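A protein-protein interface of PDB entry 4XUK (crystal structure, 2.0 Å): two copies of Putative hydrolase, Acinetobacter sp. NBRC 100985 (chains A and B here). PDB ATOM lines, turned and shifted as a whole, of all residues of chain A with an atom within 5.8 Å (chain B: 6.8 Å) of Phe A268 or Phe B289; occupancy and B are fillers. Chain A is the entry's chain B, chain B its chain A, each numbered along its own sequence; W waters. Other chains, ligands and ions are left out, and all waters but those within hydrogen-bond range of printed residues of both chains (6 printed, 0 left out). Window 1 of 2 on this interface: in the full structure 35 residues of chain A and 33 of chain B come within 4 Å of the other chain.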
ATOM      1  N   GLN A   2     -24.307  38.362   4.452  1.00  0.00           N
ATOM      2  CA  GLN A   2     -24.899  37.196   5.126  1.00  0.00           C
ATOM      3  C   GLN A   2     -25.413  37.496   6.528  1.00  0.00           C
ATOM      4  O   GLN A   2     -24.848  38.330   7.239  1.00  0.00           O
ATOM      5  CB  GLN A   2     -23.923  36.011   5.160  1.00  0.00           C
ATOM      6  CG  GLN A   2     -24.500  34.734   5.816  1.00  0.00           C
ATOM      7  CD  GLN A   2     -25.717  34.160   5.067  1.00  0.00           C
ATOM      8  OE1 GLN A   2     -26.821  34.706   5.128  1.00  0.00           O
ATOM      9  NE2 GLN A   2     -25.507  33.048   4.361  1.00  0.00           N
ATOM     10  N   VAL A   3     -26.508  36.836   6.904  1.00  0.00           N
ATOM     11  CA  VAL A   3     -27.073  37.009   8.231  1.00  0.00           C
ATOM     12  C   VAL A   3     -26.052  36.562   9.263  1.00  0.00           C
ATOM     13  O   VAL A   3     -25.187  35.727   8.981  1.00  0.00           O
ATOM     14  CB  VAL A   3     -28.432  36.277   8.387  1.00  0.00           C
ATOM     15  CG1 VAL A   3     -28.265  34.749   8.476  1.00  0.00           C
ATOM     16  CG2 VAL A   3     -29.194  36.804   9.588  1.00  0.00           C
ATOM     17  N   ALA A   4     -26.101  37.177  10.436  1.00  0.00           N
ATOM     18  CA  ALA A   4     -25.151  36.833  11.487  1.00  0.00           C
ATOM     19  C   ALA A   4     -25.465  35.427  11.972  1.00  0.00           C
ATOM     20  O   ALA A   4     -26.616  34.969  11.880  1.00  0.00           O
ATOM     21  CB  ALA A   4     -25.226  37.832  12.621  1.00  0.00           C
ATOM     22  N   GLY A   5     -24.446  34.748  12.487  1.00  0.00           N
ATOM     23  CA  GLY A   5     -24.593  33.375  12.932  1.00  0.00           C
ATOM     24  C   GLY A   5     -24.992  33.221  14.389  1.00  0.00           C
ATOM     25  O   GLY A   5     -24.234  32.658  15.185  1.00  0.00           O
ATOM     26  N   TYR A   6     -26.165  33.736  14.749  1.00  0.00           N
ATOM     27  CA  TYR A   6     -26.778  33.402  16.039  1.00  0.00           C
ATOM     28  C   TYR A   6     -28.226  33.029  15.785  1.00  0.00           C
ATOM     29  O   TYR A   6     -28.814  33.468  14.787  1.00  0.00           O
ATOM     30  CB  TYR A   6     -26.679  34.549  17.061  1.00  0.00           C
ATOM     31  CG  TYR A   6     -27.490  35.783  16.733  1.00  0.00           C
ATOM     32  CD1 TYR A   6     -26.960  36.784  15.935  1.00  0.00           C
ATOM     33  CD2 TYR A   6     -28.772  35.958  17.238  1.00  0.00           C
ATOM     34  CE1 TYR A   6     -27.677  37.919  15.631  1.00  0.00           C
ATOM     35  CE2 TYR A   6     -29.505  37.111  16.938  1.00  0.00           C
ATOM     36  CZ  TYR A   6     -28.945  38.079  16.132  1.00  0.00           C
ATOM     37  OH  TYR A   6     -29.637  39.226  15.804  1.00  0.00           O
ATOM     38  N   TYR A   7     -28.792  32.201  16.660  1.00  0.00           N
ATOM     39  CA  TYR A   7     -30.210  31.832  16.563  1.00  0.00           C
ATOM     40  C   TYR A   7     -30.775  31.554  17.956  1.00  0.00           C
ATOM     41  O   TYR A   7     -30.155  30.842  18.757  1.00  0.00           O
ATOM     42  CB  TYR A   7     -30.438  30.604  15.660  1.00  0.00           C
ATOM     43  CG  TYR A   7     -31.893  30.165  15.664  1.00  0.00           C
ATOM     44  CD1 TYR A   7     -32.831  30.817  14.873  1.00  0.00           C
ATOM     45  CD2 TYR A   7     -32.336  29.135  16.495  1.00  0.00           C
ATOM     46  CE1 TYR A   7     -34.175  30.445  14.889  1.00  0.00           C
ATOM     47  CE2 TYR A   7     -33.682  28.754  16.517  1.00  0.00           C
ATOM     48  CZ  TYR A   7     -34.588  29.420  15.717  1.00  0.00           C
ATOM     49  OH  TYR A   7     -35.921  29.066  15.722  1.00  0.00           O
ATOM     50  N   ALA A  18     -27.767  29.513  19.860  1.00  0.00           N
ATOM     51  CA  ALA A  18     -26.782  28.843  19.026  1.00  0.00           C
ATOM     52  C   ALA A  18     -25.859  29.891  18.428  1.00  0.00           C
ATOM     53  O   ALA A  18     -26.325  30.919  17.929  1.00  0.00           O
ATOM     54  CB  ALA A  18     -27.475  28.074  17.935  1.00  0.00           C
ATOM     55  N   LEU A  19     -24.555  29.633  18.476  1.00  0.00           N
ATOM     56  CA  LEU A  19     -23.561  30.577  17.986  1.00  0.00           C
ATOM     57  C   LEU A  19     -22.628  29.886  16.998  1.00  0.00           C
ATOM     58  O   LEU A  19     -22.035  28.854  17.320  1.00  0.00           O
ATOM     59  CB  LEU A  19     -22.737  31.114  19.159  1.00  0.00           C
ATOM     60  CG  LEU A  19     -23.464  31.907  20.245  1.00  0.00           C
ATOM     61  CD1 LEU A  19     -22.509  32.261  21.389  1.00  0.00           C
ATOM     62  CD2 LEU A  19     -24.099  33.160  19.646  1.00  0.00           C
ATOM     63  N   LEU A  20     -22.489  30.453  15.800  1.00  0.00           N
ATOM     64  CA  LEU A  20     -21.640  29.849  14.776  1.00  0.00           C
ATOM     65  C   LEU A  20     -20.186  30.296  14.924  1.00  0.00           C
ATOM     66  O   LEU A  20     -19.913  31.496  15.073  1.00  0.00           O
ATOM     67  CB  LEU A  20     -22.169  30.190  13.380  1.00  0.00           C
ATOM     68  CG  LEU A  20     -21.385  29.624  12.193  1.00  0.00           C
ATOM     69  CD1 LEU A  20     -21.367  28.091  12.243  1.00  0.00           C
ATOM     70  CD2 LEU A  20     -21.969  30.118  10.881  1.00  0.00           C
ATOM     71  N   THR A  23     -17.151  27.315   9.468  1.00  0.00           N
ATOM     72  CA  THR A  23     -17.543  26.131   8.716  1.00  0.00           C
ATOM     73  C   THR A  23     -16.316  25.454   8.113  1.00  0.00           C
ATOM     74  O   THR A  23     -15.503  26.104   7.443  1.00  0.00           O
ATOM     75  CB  THR A  23     -18.540  26.492   7.586  1.00  0.00           C
ATOM     76  OG1 THR A  23     -19.720  27.087   8.145  1.00  0.00           O
ATOM     77  CG2 THR A  23     -18.952  25.254   6.838  1.00  0.00           C
ATOM     78  N   GLN A  55     -19.138  19.626   4.102  1.00  0.00           N
ATOM     79  CA  GLN A  55     -19.420  20.816   4.903  1.00  0.00           C
ATOM     80  C   GLN A  55     -19.776  20.453   6.338  1.00  0.00           C
ATOM     81  O   GLN A  55     -20.678  19.634   6.572  1.00  0.00           O
ATOM     82  CB  GLN A  55     -20.566  21.613   4.272  1.00  0.00           C
ATOM     83  CG  GLN A  55     -20.799  22.981   4.903  1.00  0.00           C
ATOM     84  CD  GLN A  55     -21.846  23.781   4.151  1.00  0.00           C
ATOM     85  OE1 GLN A  55     -22.212  23.440   3.029  1.00  0.00           O
ATOM     86  NE2 GLN A  55     -22.339  24.841   4.768  1.00  0.00           N
ATOM     87  N   SER A  57     -20.386  22.247  10.256  1.00  0.00           N
ATOM     88  CA  SER A  57     -20.469  23.442  11.092  1.00  0.00           C
ATOM     89  C   SER A  57     -19.618  23.259  12.341  1.00  0.00           C
ATOM     90  O   SER A  57     -19.341  22.125  12.749  1.00  0.00           O
ATOM     91  CB  SER A  57     -21.918  23.762  11.482  1.00  0.00           C
ATOM     92  OG  SER A  57     -22.707  24.120  10.358  1.00  0.00           O
ATOM     93  N   ASN A  59     -20.172  24.951  16.062  1.00  0.00           N
ATOM     94  CA  ASN A  59     -21.086  25.781  16.838  1.00  0.00           C
ATOM     95  C   ASN A  59     -20.726  25.804  18.320  1.00  0.00           C
ATOM     96  O   ASN A  59     -20.016  24.919  18.817  1.00  0.00           O
ATOM     97  CB  ASN A  59     -22.517  25.223  16.739  1.00  0.00           C
ATOM     98  CG  ASN A  59     -22.935  24.905  15.322  1.00  0.00           C
ATOM     99  OD1 ASN A  59     -22.658  25.666  14.402  1.00  0.00           O
ATOM    100  ND2 ASN A  59     -23.631  23.770  15.139  1.00  0.00           N
ATOM    101  N   LEU A 266     -23.293  19.633  14.083  1.00  0.00           N
ATOM    102  CA  LEU A 266     -24.435  19.455  13.189  1.00  0.00           C
ATOM    103  C   LEU A 266     -24.733  20.813  12.548  1.00  0.00           C
ATOM    104  O   LEU A 266     -24.323  21.856  13.085  1.00  0.00           O
ATOM    105  CB  LEU A 266     -25.625  18.853  13.950  1.00  0.00           C
ATOM    106  CG  LEU A 266     -25.337  17.438  14.457  1.00  0.00           C
ATOM    107  CD1 LEU A 266     -26.546  16.812  15.133  1.00  0.00           C
ATOM    108  CD2 LEU A 266     -24.838  16.530  13.345  1.00  0.00           C
ATOM    109  N   PRO A 267     -25.399  20.813  11.372  1.00  0.00           N
ATOM    110  CA  PRO A 267     -25.576  22.056  10.612  1.00  0.00           C
ATOM    111  C   PRO A 267     -26.194  23.167  11.456  1.00  0.00           C
ATOM    112  O   PRO A 267     -27.274  22.958  12.009  1.00  0.00           O
ATOM    113  CB  PRO A 267     -26.533  21.636   9.488  1.00  0.00           C
ATOM    114  CG  PRO A 267     -26.179  20.197   9.248  1.00  0.00           C
ATOM    115  CD  PRO A 267     -25.899  19.638  10.629  1.00  0.00           C
ATOM    116  N   PHE A 268     -25.502  24.301  11.576  1.00  0.00           N
ATOM    117  CA  PHE A 268     -25.995  25.446  12.349  1.00  0.00           C
ATOM    118  C   PHE A 268     -27.477  25.740  12.078  1.00  0.00           C
ATOM    119  O   PHE A 268     -27.894  25.822  10.919  1.00  0.00           O
ATOM    120  CB  PHE A 268     -25.175  26.692  12.011  1.00  0.00           C
ATOM    121  CG  PHE A 268     -25.603  27.917  12.769  1.00  0.00           C
ATOM    122  CD1 PHE A 268     -25.111  28.164  14.051  1.00  0.00           C
ATOM    123  CD2 PHE A 268     -26.505  28.818  12.211  1.00  0.00           C
ATOM    124  CE1 PHE A 268     -25.516  29.291  14.764  1.00  0.00           C
ATOM    125  CE2 PHE A 268     -26.911  29.947  12.918  1.00  0.00           C
ATOM    126  CZ  PHE A 268     -26.405  30.182  14.193  1.00  0.00           C
ATOM    127  N   PRO A 269     -28.264  25.987  13.136  1.00  0.00           N
ATOM    128  CA  PRO A 269     -27.878  26.184  14.541  1.00  0.00           C
ATOM    129  C   PRO A 269     -27.575  24.917  15.348  1.00  0.00           C
ATOM    130  O   PRO A 269     -27.325  25.041  16.544  1.00  0.00           O
ATOM    131  CB  PRO A 269     -29.090  26.909  15.129  1.00  0.00           C
ATOM    132  CG  PRO A 269     -30.234  26.414  14.323  1.00  0.00           C
ATOM    133  CD  PRO A 269     -29.692  26.281  12.919  1.00  0.00           C
ATOM    134  N   GLY A 270     -27.584  23.736  14.732  1.00  0.00           N
ATOM    135  CA  GLY A 270     -27.149  22.530  15.430  1.00  0.00           C
ATOM    136  C   GLY A 270     -28.150  22.044  16.468  1.00  0.00           C
ATOM    137  O   GLY A 270     -27.820  21.228  17.346  1.00  0.00           O
ATOM    138  N   ILE A 271     -29.383  22.532  16.358  1.00  0.00           N
ATOM    139  CA  ILE A 271     -30.449  22.132  17.282  1.00  0.00           C
ATOM    140  C   ILE A 271     -31.550  21.357  16.560  1.00  0.00           C
ATOM    141  O   ILE A 271     -31.995  21.740  15.471  1.00  0.00           O
ATOM    142  CB  ILE A 271     -31.063  23.362  17.995  1.00  0.00           C
ATOM    143  CG1 ILE A 271     -29.963  24.184  18.682  1.00  0.00           C
ATOM    144  CG2 ILE A 271     -32.126  22.939  19.004  1.00  0.00           C
ATOM    145  CD1 ILE A 271     -30.436  25.550  19.197  1.00  0.00           C
ATOM    146  N   TYR B   6     -33.703  36.875   7.420  1.00  0.00           N
ATOM    147  CA  TYR B   6     -33.213  36.845   6.050  1.00  0.00           C
ATOM    148  C   TYR B   6     -32.050  35.879   6.006  1.00  0.00           C
ATOM    149  O   TYR B   6     -31.413  35.624   7.035  1.00  0.00           O
ATOM    150  CB  TYR B   6     -32.799  38.237   5.546  1.00  0.00           C
ATOM    151  CG  TYR B   6     -31.607  38.829   6.249  1.00  0.00           C
ATOM    152  CD1 TYR B   6     -31.771  39.598   7.395  1.00  0.00           C
ATOM    153  CD2 TYR B   6     -30.317  38.642   5.756  1.00  0.00           C
ATOM    154  CE1 TYR B   6     -30.687  40.155   8.047  1.00  0.00           C
ATOM    155  CE2 TYR B   6     -29.221  39.200   6.398  1.00  0.00           C
ATOM    156  CZ  TYR B   6     -29.417  39.953   7.544  1.00  0.00           C
ATOM    157  OH  TYR B   6     -28.346  40.517   8.209  1.00  0.00           O
ATOM    158  N   TYR B   7     -31.786  35.329   4.828  1.00  0.00           N
ATOM    159  CA  TYR B   7     -30.662  34.428   4.644  1.00  0.00           C
ATOM    160  C   TYR B   7     -30.170  34.572   3.221  1.00  0.00           C
ATOM    161  O   TYR B   7     -30.978  34.671   2.290  1.00  0.00           O
ATOM    162  CB  TYR B   7     -31.061  32.969   4.921  1.00  0.00           C
ATOM    163  CG  TYR B   7     -29.894  32.032   4.681  1.00  0.00           C
ATOM    164  CD1 TYR B   7     -28.935  31.825   5.666  1.00  0.00           C
ATOM    165  CD2 TYR B   7     -29.722  31.401   3.454  1.00  0.00           C
ATOM    166  CE1 TYR B   7     -27.848  30.988   5.446  1.00  0.00           C
ATOM    167  CE2 TYR B   7     -28.642  30.575   3.222  1.00  0.00           C
ATOM    168  CZ  TYR B   7     -27.715  30.372   4.226  1.00  0.00           C
ATOM    169  OH  TYR B   7     -26.634  29.556   4.002  1.00  0.00           O
ATOM    170  N   PRO B 286     -32.861  20.500   3.760  1.00  0.00           N
ATOM    171  CA  PRO B 286     -32.583  21.943   3.791  1.00  0.00           C
ATOM    172  C   PRO B 286     -31.120  22.242   3.446  1.00  0.00           C
ATOM    173  O   PRO B 286     -30.239  21.397   3.643  1.00  0.00           O
ATOM    174  CB  PRO B 286     -32.902  22.339   5.244  1.00  0.00           C
ATOM    175  CG  PRO B 286     -32.817  21.064   6.028  1.00  0.00           C
ATOM    176  CD  PRO B 286     -33.229  19.963   5.084  1.00  0.00           C
ATOM    177  N   ILE B 287     -30.852  23.417   2.893  1.00  0.00           N
ATOM    178  CA  ILE B 287     -29.460  23.754   2.612  1.00  0.00           C
ATOM    179  C   ILE B 287     -28.712  23.947   3.920  1.00  0.00           C
ATOM    180  O   ILE B 287     -29.322  24.177   4.973  1.00  0.00           O
ATOM    181  CB  ILE B 287     -29.308  24.998   1.734  1.00  0.00           C
ATOM    182  CG1 ILE B 287     -30.134  26.155   2.288  1.00  0.00           C
ATOM    183  CG2 ILE B 287     -29.718  24.692   0.302  1.00  0.00           C
ATOM    184  CD1 ILE B 287     -29.296  27.356   2.595  1.00  0.00           C
ATOM    185  N   HIS B 288     -27.392  23.835   3.847  1.00  0.00           N
ATOM    186  CA  HIS B 288     -26.541  23.860   5.030  1.00  0.00           C
ATOM    187  C   HIS B 288     -26.002  25.290   5.165  1.00  0.00           C
ATOM    188  O   HIS B 288     -25.330  25.787   4.254  1.00  0.00           O
ATOM    189  CB  HIS B 288     -25.405  22.840   4.835  1.00  0.00           C
ATOM    190  CG  HIS B 288     -24.557  22.607   6.052  1.00  0.00           C
ATOM    191  ND1 HIS B 288     -23.858  21.434   6.258  1.00  0.00           N
ATOM    192  CD2 HIS B 288     -24.285  23.396   7.118  1.00  0.00           C
ATOM    193  CE1 HIS B 288     -23.202  21.507   7.402  1.00  0.00           C
ATOM    194  NE2 HIS B 288     -23.441  22.688   7.944  1.00  0.00           N
ATOM    195  N   PHE B 289     -26.347  25.978   6.237  1.00  0.00           N
ATOM    196  CA  PHE B 289     -25.907  27.350   6.534  1.00  0.00           C
ATOM    197  C   PHE B 289     -24.452  27.665   6.101  1.00  0.00           C
ATOM    198  O   PHE B 289     -23.526  26.913   6.547  1.00  0.00           O
ATOM    199  CB  PHE B 289     -26.112  27.666   8.029  1.00  0.00           C
ATOM    200  CG  PHE B 289     -26.026  29.127   8.371  1.00  0.00           C
ATOM    201  CD1 PHE B 289     -24.825  29.797   8.330  1.00  0.00           C
ATOM    202  CD2 PHE B 289     -27.125  29.830   8.707  1.00  0.00           C
ATOM    203  CE1 PHE B 289     -24.743  31.122   8.619  1.00  0.00           C
ATOM    204  CE2 PHE B 289     -27.047  31.155   8.991  1.00  0.00           C
ATOM    205  CZ  PHE B 289     -25.848  31.805   8.944  1.00  0.00           C
ATOM    206  N   LYS B 290     -24.267  28.682   5.316  1.00  0.00           N
ATOM    207  CA  LYS B 290     -22.971  29.050   4.900  1.00  0.00           C
ATOM    208  C   LYS B 290     -22.582  30.492   5.295  1.00  0.00           C
ATOM    209  O   LYS B 290     -23.141  31.421   4.824  1.00  0.00           O
ATOM    210  CB  LYS B 290     -22.892  28.847   3.429  1.00  0.00           C
ATOM    211  CG  LYS B 290     -21.578  28.345   2.903  1.00  0.00           C
ATOM    212  CD  LYS B 290     -21.765  27.891   1.480  1.00  0.00           C
ATOM    213  CE  LYS B 290     -21.106  26.562   1.172  1.00  0.00           C
ATOM    214  NZ  LYS B 290     -21.968  25.494   0.587  1.00  0.00           N
ATOM    215  N   ASP B 291     -21.692  30.612   6.240  1.00  0.00           N
ATOM    216  CA  ASP B 291     -21.157  31.881   6.583  1.00  0.00           C
ATOM    217  C   ASP B 291     -20.124  32.121   5.524  1.00  0.00           C
ATOM    218  O   ASP B 291     -19.922  33.205   5.208  1.00  0.00           O
ATOM    219  CB  ASP B 291     -20.542  31.896   7.979  1.00  0.00           C
ATOM    220  CG  ASP B 291     -19.370  30.933   8.119  1.00  0.00           C
ATOM    221  OD1 ASP B 291     -19.457  29.812   7.639  1.00  0.00           O
ATOM    222  OD2 ASP B 291     -18.373  31.325   8.674  1.00  0.00           O
HETATM  223  O   HOH W   1     -27.252  24.503   8.510  1.00  0.00           O
HETATM  224  O   HOH W   2     -25.942  40.637   7.300  1.00  0.00           O
HETATM  225  O   HOH W   3     -22.469  20.455  10.395  1.00  0.00           O
HETATM  226  O   HOH W   4     -22.058  25.906   8.470  1.00  0.00           O
HETATM  227  O   HOH W   5     -16.136  29.550   8.006  1.00  0.00           O
HETATM  228  O   HOH W   6     -27.657  39.604  11.029  1.00  0.00           O
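O of Phe B289 is in hydrogen-bond range of NE2 of Gln A55. NE2 of Gln A55 is in hydrogen-bond range of O of His B288. The backbone carbonyl oxygen of Lys B290 lies within hydrogen-bond range of the side-chain amide nitrogen of Gln A2 (2.9 Å). The side-chain amide oxygen of Gln A55 is in hydrogen-bond range of the side-chain amino group of Lys B290 (3.2 Å). NE2 of His B288 is in hydrogen-bond range of OG of Ser A57 (2.9 Å). The side-chain carboxylate (OD1) of Asp B291 lies within hydrogen-bond range of the side-chain hydroxyl (OG1) of Thr A23 (2.8 Å).
The side-chain hydroxyl (OH) of Tyr B7 is in hydrogen-bond range of the backbone NH (N) of Lys B290, 2.8 Å away. N of Leu A20 sits at hydrogen-bond distance from O of Gly A5 (2.9 Å). The side-chain hydroxyl of Ser A57 lies within hydrogen-bond range of the backbone NH of Phe A268 (3.1 Å).
Tyr B7 touches Gln A2. CB of Val A3 touches O of Tyr B6, 3.3 Å away. Val A3 touches Phe B289. CD2 of Leu A20 touches CE1 of Phe B289, at 3.7 Å. Leu A20 touches Asp B291 (CD2 to CB, 3.7 Å). Pro A267 touches His B288. Phe B289 touches Phe A268 (CD2 to CD2, 3.7 Å).
Of the printed residues of chain B, Val A3 touches Tyr B6 and Phe B289. Of the printed residues of chain B, Ser A57 touches His B288. Phe A268 touches one residue of chain B. Pro A269 touches none of the printed residues of chain B. Gly A270 touches none of the printed residues of chain B. Of the printed residues of chain A, Phe B289 touches Val A3 (3.8 Å), Leu A20 (3.7 Å), Gln A55 (3.0 Å) and Phe A268 (3.7 Å). The nearest printed residue of chain B that does not touch Thr A23 is Phe B289 (4.1 Å).
Printed residues of chain A that touch a printed residue of chain B: Gln A2, Val A3, Leu A20, Thr A23, Gln A55, Ser A57, Pro A267 and Phe A268. Hydrophobic or aromatic side chains of chain A within 4 Å of the printed part of chain B: Val A3, Leu A20, Pro A267 and Phe A268. Of the 8 printed residues of chain B, 6 touch a printed residue of chain A. Hydrophobic or aromatic side chains of chain B that line the printed part of chain A: Tyr B6, Tyr B7, His B288 and Phe B289.
Positions printed for both chains: 6 and 7. Of the 13 pairs that touch across the chains among the printed residues, none has its exchanged pair printed and touching as well.
Water W2 bridges O of Gln A2 (2.6 Å) and OH of Tyr B6 (2.6 Å). Water W4 lies within hydrogen-bond range of the backbone carbonyl oxygen (O) of Phe B289 (2.6 Å), the side-chain hydroxyl (OG1) of Thr A23 (2.6 Å) and the side-chain hydroxyl (OG) of Ser A57 (2.7 Å). Water W3 lies within hydrogen-bond range of the backbone NH (N) of Ser A57 and a ring nitrogen (NE2) of His B288. Water W1 lies within hydrogen-bond range of O of Phe A268 and N of Phe B289. Water W5 lies within hydrogen-bond range of the backbone NH (N) of Thr A23 and the side-chain carboxylate (OD2) of Asp B291. Water W6 bridges N of Ala A4 (2.9 Å) and OH of Tyr B6 (3.0 Å).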
